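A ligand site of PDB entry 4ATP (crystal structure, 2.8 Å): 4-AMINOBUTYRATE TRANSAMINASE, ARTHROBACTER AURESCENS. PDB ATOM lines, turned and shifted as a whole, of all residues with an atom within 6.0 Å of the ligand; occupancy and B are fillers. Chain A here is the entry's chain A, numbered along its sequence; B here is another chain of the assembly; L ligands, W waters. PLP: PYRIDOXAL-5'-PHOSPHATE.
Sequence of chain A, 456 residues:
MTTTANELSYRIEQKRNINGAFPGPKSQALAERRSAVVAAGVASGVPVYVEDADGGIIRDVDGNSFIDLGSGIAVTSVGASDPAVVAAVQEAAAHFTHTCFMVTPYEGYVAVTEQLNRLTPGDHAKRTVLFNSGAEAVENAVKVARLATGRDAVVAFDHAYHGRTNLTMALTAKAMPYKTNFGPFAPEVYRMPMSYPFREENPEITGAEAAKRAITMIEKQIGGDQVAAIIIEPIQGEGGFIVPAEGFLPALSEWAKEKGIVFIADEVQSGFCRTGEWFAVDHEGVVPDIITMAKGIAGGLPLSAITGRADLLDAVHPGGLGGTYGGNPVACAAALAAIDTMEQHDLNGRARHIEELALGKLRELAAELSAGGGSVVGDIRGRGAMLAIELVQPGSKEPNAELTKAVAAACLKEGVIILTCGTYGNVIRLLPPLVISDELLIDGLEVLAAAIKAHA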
ATOM      1  N   ILE A  73     -35.858 -25.108  -4.917  1.00  0.00           N
ATOM      2  CA  ILE A  73     -34.611 -25.366  -4.197  1.00  0.00           C
ATOM      3  C   ILE A  73     -33.628 -24.206  -4.405  1.00  0.00           C
ATOM      4  O   ILE A  73     -32.559 -24.375  -4.961  1.00  0.00           O
ATOM      5  CB  ILE A  73     -33.918 -26.699  -4.502  1.00  0.00           C
ATOM      6  CG1 ILE A  73     -34.934 -27.836  -4.726  1.00  0.00           C
ATOM      7  CG2 ILE A  73     -32.999 -26.998  -3.351  1.00  0.00           C
ATOM      8  CD1 ILE A  73     -34.361 -29.212  -5.086  1.00  0.00           C
ATOM      9  N   ASN A 132     -23.169 -25.503 -16.991  1.00  0.00           N
ATOM     10  CA  ASN A 132     -24.626 -25.568 -16.872  1.00  0.00           C
ATOM     11  C   ASN A 132     -25.103 -25.864 -15.471  1.00  0.00           C
ATOM     12  O   ASN A 132     -25.930 -25.116 -14.984  1.00  0.00           O
ATOM     13  CB  ASN A 132     -25.140 -26.616 -17.829  1.00  0.00           C
ATOM     14  CG  ASN A 132     -24.482 -26.481 -19.188  1.00  0.00           C
ATOM     15  OD1 ASN A 132     -24.775 -25.544 -19.939  1.00  0.00           O
ATOM     16  ND2 ASN A 132     -23.598 -27.395 -19.490  1.00  0.00           N
ATOM     17  N   SER A 133     -24.629 -26.938 -14.860  1.00  0.00           N
ATOM     18  CA  SER A 133     -25.148 -27.380 -13.550  1.00  0.00           C
ATOM     19  C   SER A 133     -24.194 -27.163 -12.397  1.00  0.00           C
ATOM     20  O   SER A 133     -22.965 -26.986 -12.586  1.00  0.00           O
ATOM     21  CB  SER A 133     -25.482 -28.864 -13.556  1.00  0.00           C
ATOM     22  OG  SER A 133     -24.310 -29.694 -13.736  1.00  0.00           O
ATOM     23  N   GLY A 134     -24.748 -27.185 -11.208  1.00  0.00           N
ATOM     24  CA  GLY A 134     -23.943 -27.066 -10.009  1.00  0.00           C
ATOM     25  C   GLY A 134     -22.902 -28.168  -9.951  1.00  0.00           C
ATOM     26  O   GLY A 134     -21.746 -27.935  -9.619  1.00  0.00           O
ATOM     27  N   ALA A 135     -23.321 -29.387 -10.260  1.00  0.00           N
ATOM     28  CA  ALA A 135     -22.392 -30.505 -10.265  1.00  0.00           C
ATOM     29  C   ALA A 135     -21.216 -30.228 -11.210  1.00  0.00           C
ATOM     30  O   ALA A 135     -20.073 -30.482 -10.870  1.00  0.00           O
ATOM     31  CB  ALA A 135     -23.079 -31.803 -10.617  1.00  0.00           C
ATOM     32  N   GLU A 136     -21.514 -29.692 -12.374  1.00  0.00           N
ATOM     33  CA  GLU A 136     -20.437 -29.393 -13.318  1.00  0.00           C
ATOM     34  C   GLU A 136     -19.505 -28.328 -12.689  1.00  0.00           C
ATOM     35  O   GLU A 136     -18.275 -28.409 -12.866  1.00  0.00           O
ATOM     36  CB  GLU A 136     -20.994 -28.948 -14.671  1.00  0.00           C
ATOM     37  CG  GLU A 136     -21.518 -30.087 -15.524  1.00  0.00           C
ATOM     38  CD  GLU A 136     -22.009 -29.605 -16.916  1.00  0.00           C
ATOM     39  OE1 GLU A 136     -22.698 -28.537 -16.958  1.00  0.00           O
ATOM     40  OE2 GLU A 136     -21.699 -30.293 -17.938  1.00  0.00           O
ATOM     41  N   VAL A 138     -18.832 -27.800  -9.479  1.00  0.00           N
ATOM     42  CA  VAL A 138     -17.994 -28.461  -8.487  1.00  0.00           C
ATOM     43  C   VAL A 138     -16.931 -29.350  -9.134  1.00  0.00           C
ATOM     44  O   VAL A 138     -15.764 -29.297  -8.774  1.00  0.00           O
ATOM     45  CB  VAL A 138     -18.810 -29.276  -7.493  1.00  0.00           C
ATOM     46  CG1 VAL A 138     -17.873 -30.076  -6.586  1.00  0.00           C
ATOM     47  CG2 VAL A 138     -19.705 -28.329  -6.696  1.00  0.00           C
ATOM     48  N   TYR A 161     -23.242 -31.945   0.689  1.00  0.00           N
ATOM     49  CA  TYR A 161     -23.907 -32.348  -0.556  1.00  0.00           C
ATOM     50  C   TYR A 161     -23.328 -31.515  -1.679  1.00  0.00           C
ATOM     51  O   TYR A 161     -23.324 -30.274  -1.580  1.00  0.00           O
ATOM     52  CB  TYR A 161     -25.426 -32.131  -0.486  1.00  0.00           C
ATOM     53  CG  TYR A 161     -26.042 -32.474  -1.816  1.00  0.00           C
ATOM     54  CD1 TYR A 161     -26.358 -33.776  -2.152  1.00  0.00           C
ATOM     55  CD2 TYR A 161     -26.239 -31.487  -2.773  1.00  0.00           C
ATOM     56  CE1 TYR A 161     -26.887 -34.087  -3.381  1.00  0.00           C
ATOM     57  CE2 TYR A 161     -26.769 -31.798  -4.011  1.00  0.00           C
ATOM     58  CZ  TYR A 161     -27.084 -33.094  -4.317  1.00  0.00           C
ATOM     59  OH  TYR A 161     -27.597 -33.396  -5.558  1.00  0.00           O
ATOM     60  N   HIS A 162     -22.881 -32.154  -2.751  1.00  0.00           N
ATOM     61  CA  HIS A 162     -22.260 -31.405  -3.860  1.00  0.00           C
ATOM     62  C   HIS A 162     -22.702 -31.841  -5.221  1.00  0.00           C
ATOM     63  O   HIS A 162     -22.197 -31.333  -6.214  1.00  0.00           O
ATOM     64  CB  HIS A 162     -20.721 -31.485  -3.785  1.00  0.00           C
ATOM     65  CG  HIS A 162     -20.132 -30.917  -2.528  1.00  0.00           C
ATOM     66  ND1 HIS A 162     -20.044 -29.608  -2.303  1.00  0.00           N
ATOM     67  CD2 HIS A 162     -19.623 -31.553  -1.393  1.00  0.00           C
ATOM     68  CE1 HIS A 162     -19.520 -29.407  -1.086  1.00  0.00           C
ATOM     69  NE2 HIS A 162     -19.265 -30.602  -0.531  1.00  0.00           N
ATOM     70  N   GLY A 163     -23.588 -32.820  -5.327  1.00  0.00           N
ATOM     71  CA  GLY A 163     -24.112 -33.228  -6.619  1.00  0.00           C
ATOM     72  C   GLY A 163     -24.230 -34.704  -6.918  1.00  0.00           C
ATOM     73  O   GLY A 163     -23.863 -35.551  -6.119  1.00  0.00           O
ATOM     74  N   ARG A 164     -24.669 -34.990  -8.130  1.00  0.00           N
ATOM     75  CA  ARG A 164     -25.082 -36.313  -8.523  1.00  0.00           C
ATOM     76  C   ARG A 164     -24.271 -36.934  -9.647  1.00  0.00           C
ATOM     77  O   ARG A 164     -24.629 -38.024 -10.136  1.00  0.00           O
ATOM     78  CB  ARG A 164     -26.546 -36.262  -8.910  1.00  0.00           C
ATOM     79  CG  ARG A 164     -27.512 -36.037  -7.762  1.00  0.00           C
ATOM     80  CD  ARG A 164     -28.921 -35.938  -8.328  1.00  0.00           C
ATOM     81  NE  ARG A 164     -29.926 -35.578  -7.342  1.00  0.00           N
ATOM     82  CZ  ARG A 164     -30.712 -36.454  -6.708  1.00  0.00           C
ATOM     83  NH1 ARG A 164     -30.622 -37.769  -6.955  1.00  0.00           N
ATOM     84  NH2 ARG A 164     -31.608 -36.001  -5.833  1.00  0.00           N
ATOM     85  N   GLU A 233     -19.429 -26.171   2.023  1.00  0.00           N
ATOM     86  CA  GLU A 233     -20.537 -25.252   1.895  1.00  0.00           C
ATOM     87  C   GLU A 233     -20.524 -24.386   3.146  1.00  0.00           C
ATOM     88  O   GLU A 233     -20.570 -24.912   4.260  1.00  0.00           O
ATOM     89  CB  GLU A 233     -21.854 -26.028   1.868  1.00  0.00           C
ATOM     90  CG  GLU A 233     -21.971 -27.098   0.797  1.00  0.00           C
ATOM     91  CD  GLU A 233     -23.104 -28.063   1.083  1.00  0.00           C
ATOM     92  OE1 GLU A 233     -24.276 -27.654   0.909  1.00  0.00           O
ATOM     93  OE2 GLU A 233     -22.818 -29.223   1.474  1.00  0.00           O
ATOM     94  N   GLY A 237     -26.459 -27.173   2.732  1.00  0.00           N
ATOM     95  CA  GLY A 237     -27.870 -27.177   2.298  1.00  0.00           C
ATOM     96  C   GLY A 237     -28.637 -28.439   2.608  1.00  0.00           C
ATOM     97  O   GLY A 237     -29.245 -28.563   3.684  1.00  0.00           O
ATOM     98  N   GLU A 238     -28.560 -29.406   1.688  1.00  0.00           N
ATOM     99  CA  GLU A 238     -29.265 -30.670   1.865  1.00  0.00           C
ATOM    100  C   GLU A 238     -28.917 -31.368   3.175  1.00  0.00           C
ATOM    101  O   GLU A 238     -29.701 -32.134   3.708  1.00  0.00           O
ATOM    102  CB  GLU A 238     -28.983 -31.598   0.698  1.00  0.00           C
ATOM    103  CG  GLU A 238     -29.201 -30.983  -0.686  1.00  0.00           C
ATOM    104  CD  GLU A 238     -30.596 -30.392  -0.882  1.00  0.00           C
ATOM    105  OE1 GLU A 238     -31.580 -31.151  -0.854  1.00  0.00           O
ATOM    106  OE2 GLU A 238     -30.682 -29.173  -1.056  1.00  0.00           O
ATOM    107  N   ASP A 266     -18.379 -23.976  -1.768  1.00  0.00           N
ATOM    108  CA  ASP A 266     -19.545 -24.341  -2.593  1.00  0.00           C
ATOM    109  C   ASP A 266     -20.751 -23.483  -2.230  1.00  0.00           C
ATOM    110  O   ASP A 266     -21.451 -23.774  -1.260  1.00  0.00           O
ATOM    111  CB  ASP A 266     -19.892 -25.811  -2.473  1.00  0.00           C
ATOM    112  CG  ASP A 266     -20.927 -26.239  -3.472  1.00  0.00           C
ATOM    113  OD1 ASP A 266     -21.468 -25.382  -4.209  1.00  0.00           O
ATOM    114  OD2 ASP A 266     -21.186 -27.460  -3.574  1.00  0.00           O
ATOM    115  N   GLU A 267     -20.978 -22.440  -3.033  1.00  0.00           N
ATOM    116  CA  GLU A 267     -22.070 -21.483  -2.802  1.00  0.00           C
ATOM    117  C   GLU A 267     -23.190 -21.673  -3.850  1.00  0.00           C
ATOM    118  O   GLU A 267     -23.869 -20.714  -4.224  1.00  0.00           O
ATOM    119  CB  GLU A 267     -21.539 -20.054  -2.857  1.00  0.00           C
ATOM    120  CG  GLU A 267     -20.573 -19.728  -1.725  1.00  0.00           C
ATOM    121  CD  GLU A 267     -21.158 -18.803  -0.668  1.00  0.00           C
ATOM    122  OE1 GLU A 267     -22.397 -18.575  -0.636  1.00  0.00           O
ATOM    123  OE2 GLU A 267     -20.361 -18.237   0.103  1.00  0.00           O
ATOM    124  N   VAL A 268     -23.364 -22.892  -4.335  1.00  0.00           N
ATOM    125  CA  VAL A 268     -24.397 -23.156  -5.316  1.00  0.00           C
ATOM    126  C   VAL A 268     -25.764 -22.822  -4.748  1.00  0.00           C
ATOM    127  O   VAL A 268     -26.579 -22.221  -5.435  1.00  0.00           O
ATOM    128  CB  VAL A 268     -24.361 -24.595  -5.853  1.00  0.00           C
ATOM    129  CG1 VAL A 268     -25.758 -25.027  -6.287  1.00  0.00           C
ATOM    130  CG2 VAL A 268     -23.369 -24.669  -7.019  1.00  0.00           C
ATOM    131  N   GLN A 269     -26.020 -23.200  -3.499  1.00  0.00           N
ATOM    132  CA  GLN A 269     -27.324 -22.954  -2.850  1.00  0.00           C
ATOM    133  C   GLN A 269     -27.328 -21.653  -2.048  1.00  0.00           C
ATOM    134  O   GLN A 269     -28.300 -20.909  -2.108  1.00  0.00           O
ATOM    135  CB  GLN A 269     -27.715 -24.127  -1.953  1.00  0.00           C
ATOM    136  CG  GLN A 269     -29.146 -24.041  -1.402  1.00  0.00           C
ATOM    137  CD  GLN A 269     -29.648 -25.356  -0.777  1.00  0.00           C
ATOM    138  OE1 GLN A 269     -30.440 -25.339   0.173  1.00  0.00           O
ATOM    139  NE2 GLN A 269     -29.178 -26.490  -1.306  1.00  0.00           N
ATOM    140  N   THR A 292     -17.864 -21.974  -6.212  1.00  0.00           N
ATOM    141  CA  THR A 292     -18.749 -22.612  -7.159  1.00  0.00           C
ATOM    142  C   THR A 292     -20.147 -22.020  -7.017  1.00  0.00           C
ATOM    143  O   THR A 292     -20.682 -21.888  -5.895  1.00  0.00           O
ATOM    144  CB  THR A 292     -18.828 -24.140  -6.980  1.00  0.00           C
ATOM    145  OG1 THR A 292     -19.261 -24.477  -5.664  1.00  0.00           O
ATOM    146  CG2 THR A 292     -17.489 -24.789  -7.190  1.00  0.00           C
ATOM    147  N   ALA A 294     -24.304 -21.777  -8.896  1.00  0.00           N
ATOM    148  CA  ALA A 294     -25.366 -22.175  -9.825  1.00  0.00           C
ATOM    149  C   ALA A 294     -26.732 -21.689  -9.292  1.00  0.00           C
ATOM    150  O   ALA A 294     -26.838 -20.568  -8.830  1.00  0.00           O
ATOM    151  CB  ALA A 294     -25.350 -23.697 -10.031  1.00  0.00           C
ATOM    152  N   LYS A 295     -27.755 -22.551  -9.340  1.00  0.00           N
ATOM    153  CA  LYS A 295     -29.090 -22.267  -8.785  1.00  0.00           C
ATOM    154  C   LYS A 295     -29.539 -20.795  -9.039  1.00  0.00           C
ATOM    155  O   LYS A 295     -29.973 -20.453 -10.149  1.00  0.00           O
ATOM    156  CB  LYS A 295     -29.171 -22.737  -7.290  1.00  0.00           C
ATOM    157  CG  LYS A 295     -29.248 -24.283  -7.073  1.00  0.00           C
ATOM    158  CD  LYS A 295     -29.279 -24.771  -5.600  1.00  0.00           C
ATOM    159  CE  LYS A 295     -29.776 -26.220  -5.359  1.00  0.00           C
ATOM    160  NZ  LYS A 295     -28.528 -27.020  -5.345  1.00  0.00           N
ATOM    161  N   ASN B 132     -29.323 -31.695 -17.976  1.00  0.00           N
ATOM    162  CA  ASN B 132     -28.895 -30.507 -18.694  1.00  0.00           C
ATOM    163  C   ASN B 132     -27.862 -30.829 -19.753  1.00  0.00           C
ATOM    164  O   ASN B 132     -28.052 -30.424 -20.910  1.00  0.00           O
ATOM    165  CB  ASN B 132     -28.355 -29.485 -17.714  1.00  0.00           C
ATOM    166  CG  ASN B 132     -29.257 -29.310 -16.512  1.00  0.00           C
ATOM    167  OD1 ASN B 132     -30.342 -28.769 -16.646  1.00  0.00           O
ATOM    168  ND2 ASN B 132     -28.835 -29.778 -15.352  1.00  0.00           N
ATOM    169  N   GLU B 136     -23.890 -35.154 -18.149  1.00  0.00           N
ATOM    170  CA  GLU B 136     -24.855 -35.603 -17.149  1.00  0.00           C
ATOM    171  C   GLU B 136     -25.661 -36.811 -17.664  1.00  0.00           C
ATOM    172  O   GLU B 136     -25.955 -37.763 -16.932  1.00  0.00           O
ATOM    173  CB  GLU B 136     -25.776 -34.462 -16.723  1.00  0.00           C
ATOM    174  CG  GLU B 136     -25.132 -33.462 -15.795  1.00  0.00           C
ATOM    175  CD  GLU B 136     -26.090 -32.377 -15.338  1.00  0.00           C
ATOM    176  OE1 GLU B 136     -26.834 -31.848 -16.178  1.00  0.00           O
ATOM    177  OE2 GLU B 136     -26.091 -32.026 -14.102  1.00  0.00           O
ATOM    178  N   GLY B 323     -31.323 -33.822 -10.288  1.00  0.00           N
ATOM    179  CA  GLY B 323     -30.657 -32.561 -10.601  1.00  0.00           C
ATOM    180  C   GLY B 323     -31.620 -31.387 -10.388  1.00  0.00           C
ATOM    181  O   GLY B 323     -32.835 -31.568 -10.376  1.00  0.00           O
ATOM    182  N   THR B 324     -31.091 -30.189 -10.173  1.00  0.00           N
ATOM    183  CA  THR B 324     -31.927 -29.019  -9.933  1.00  0.00           C
ATOM    184  C   THR B 324     -32.576 -28.527 -11.223  1.00  0.00           C
ATOM    185  O   THR B 324     -33.792 -28.476 -11.318  1.00  0.00           O
ATOM    186  CB  THR B 324     -31.079 -27.875  -9.331  1.00  0.00           C
ATOM    187  OG1 THR B 324     -30.565 -28.271  -8.047  1.00  0.00           O
ATOM    188  CG2 THR B 324     -31.895 -26.564  -9.201  1.00  0.00           C
ATOM    189  N   TYR B 325     -31.744 -28.137 -12.175  1.00  0.00           N
ATOM    190  CA  TYR B 325     -32.197 -27.502 -13.403  1.00  0.00           C
ATOM    191  C   TYR B 325     -32.843 -28.485 -14.370  1.00  0.00           C
ATOM    192  O   TYR B 325     -33.567 -28.089 -15.279  1.00  0.00           O
ATOM    193  CB  TYR B 325     -31.007 -26.899 -14.159  1.00  0.00           C
ATOM    194  CG  TYR B 325     -30.377 -25.657 -13.589  1.00  0.00           C
ATOM    195  CD1 TYR B 325     -31.133 -24.644 -13.044  1.00  0.00           C
ATOM    196  CD2 TYR B 325     -29.009 -25.469 -13.689  1.00  0.00           C
ATOM    197  CE1 TYR B 325     -30.563 -23.473 -12.594  1.00  0.00           C
ATOM    198  CE2 TYR B 325     -28.427 -24.301 -13.252  1.00  0.00           C
ATOM    199  CZ  TYR B 325     -29.205 -23.295 -12.723  1.00  0.00           C
ATOM    200  OH  TYR B 325     -28.625 -22.126 -12.296  1.00  0.00           O
HETATM  201  N1  PLP L   1     -23.712 -28.150  -4.490  1.00  0.00           N
HETATM  202  C2  PLP L   1     -24.586 -27.675  -3.627  1.00  0.00           C
HETATM  203  C2A PLP L   1     -24.064 -27.121  -2.339  1.00  0.00           C
HETATM  204  C3  PLP L   1     -26.039 -27.698  -3.943  1.00  0.00           C
HETATM  205  O3  PLP L   1     -26.935 -27.210  -3.023  1.00  0.00           O
HETATM  206  C4  PLP L   1     -26.516 -28.293  -5.203  1.00  0.00           C
HETATM  207  C4A PLP L   1     -27.968 -28.167  -5.656  1.00  0.00           C
HETATM  208  C5  PLP L   1     -25.429 -28.733  -6.100  1.00  0.00           C
HETATM  209  C6  PLP L   1     -24.107 -28.658  -5.663  1.00  0.00           C
HETATM  210  C5A PLP L   1     -25.675 -29.364  -7.436  1.00  0.00           C
HETATM  211  O4P PLP L   1     -26.304 -28.482  -8.338  1.00  0.00           O
HETATM  212  P   PLP L   1     -27.121 -29.024  -9.624  1.00  0.00           P
HETATM  213  O1P PLP L   1     -27.277 -27.753 -10.341  1.00  0.00           O
HETATM  214  O2P PLP L   1     -26.202 -29.977 -10.335  1.00  0.00           O
HETATM  215  O3P PLP L   1     -28.383 -29.673  -9.084  1.00  0.00           O
HETATM  216  O   HOH W   1     -26.529 -28.540  -0.435  1.00  0.00           O
HETATM  217  O   HOH W   2     -28.460 -25.207 -10.252  1.00  0.00           O
HETATM  218  O   HOH W   3     -28.691 -28.511 -12.414  1.00  0.00           O
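An oxygen (O1P) of the ligand lies within hydrogen-bond range of the backbone NH of Gly 134 (2.7 Å). The side-chain amino group (NZ) of Lys 295 is bonded to a carbon (C4A) of the ligand, 1.3 Å away. The backbone NH (N) of Thr 324 of chain B sits at hydrogen-bond distance from an oxygen (O3P) of the ligand (3.0 Å). OG1 of Thr 324 of chain B is in hydrogen-bond range of O3P of the ligand (2.8 Å). N of Ala 135 sits at hydrogen-bond distance from O2P of the ligand (2.9 Å). The side-chain carboxylate (OD2) of Asp 266 is in hydrogen-bond range of a nitrogen (N1) of the ligand, 2.8 Å away. The side-chain amide nitrogen (NE2) of Gln 269 sits at hydrogen-bond distance from an oxygen (O3) of the ligand (2.9 Å).
OG of Ser 133 is in hydrogen-bond range of OE2 of Glu 136 of chain B. N of Gly 237 sits at hydrogen-bond distance from OE1 of Glu 233 (2.9 Å). OE2 of Glu 233 lies within hydrogen-bond range of N of Tyr 161. NE2 of Gln 269 lies within hydrogen-bond range of OE2 of Glu 238 (3.1 Å). The side-chain hydroxyl of Ser 133 is in hydrogen-bond range of the backbone NH of Glu 136 of chain A, at 3.1 Å. The backbone NH (N) of Val 268 sits at hydrogen-bond distance from the backbone carbonyl oxygen (O) of Thr 292, 3.3 Å away. ND1 of His 162 is in hydrogen-bond range of OD2 of Asp 266 (2.7 Å). The backbone carbonyl oxygen of Lys 295 is in hydrogen-bond range of the side-chain hydroxyl of Tyr 325 of chain B (3.0 Å).
Merely in contact with the ligand: Glu 233 (3.3 Å), Tyr 161 (3.3 Å), His 162 (3.3 Å), Ser 133 (3.5 Å), Val 268 (3.5 Å) and Gly 323 of chain B (3.9 Å). Hydrophobic or aromatic side chains that line the ligand: Ala 135, Tyr 161 and Val 268. Within 4 Å of the ligand: Ser 133, Gly 134, Ala 135, Tyr 161, His 162, Glu 233, Asp 266, Val 268, Gln 269, Lys 295, Gly 323 of chain B and Thr 324 of chain B.
Water W3 lies within hydrogen-bond range of O1P of the ligand (2.6 Å), N of Tyr 325 of chain B (3.1 Å) and ND2 of Asn 132 of chain B (3.2 Å). Water W2 lies within hydrogen-bond range of O1P of the ligand and N of Lys 295.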
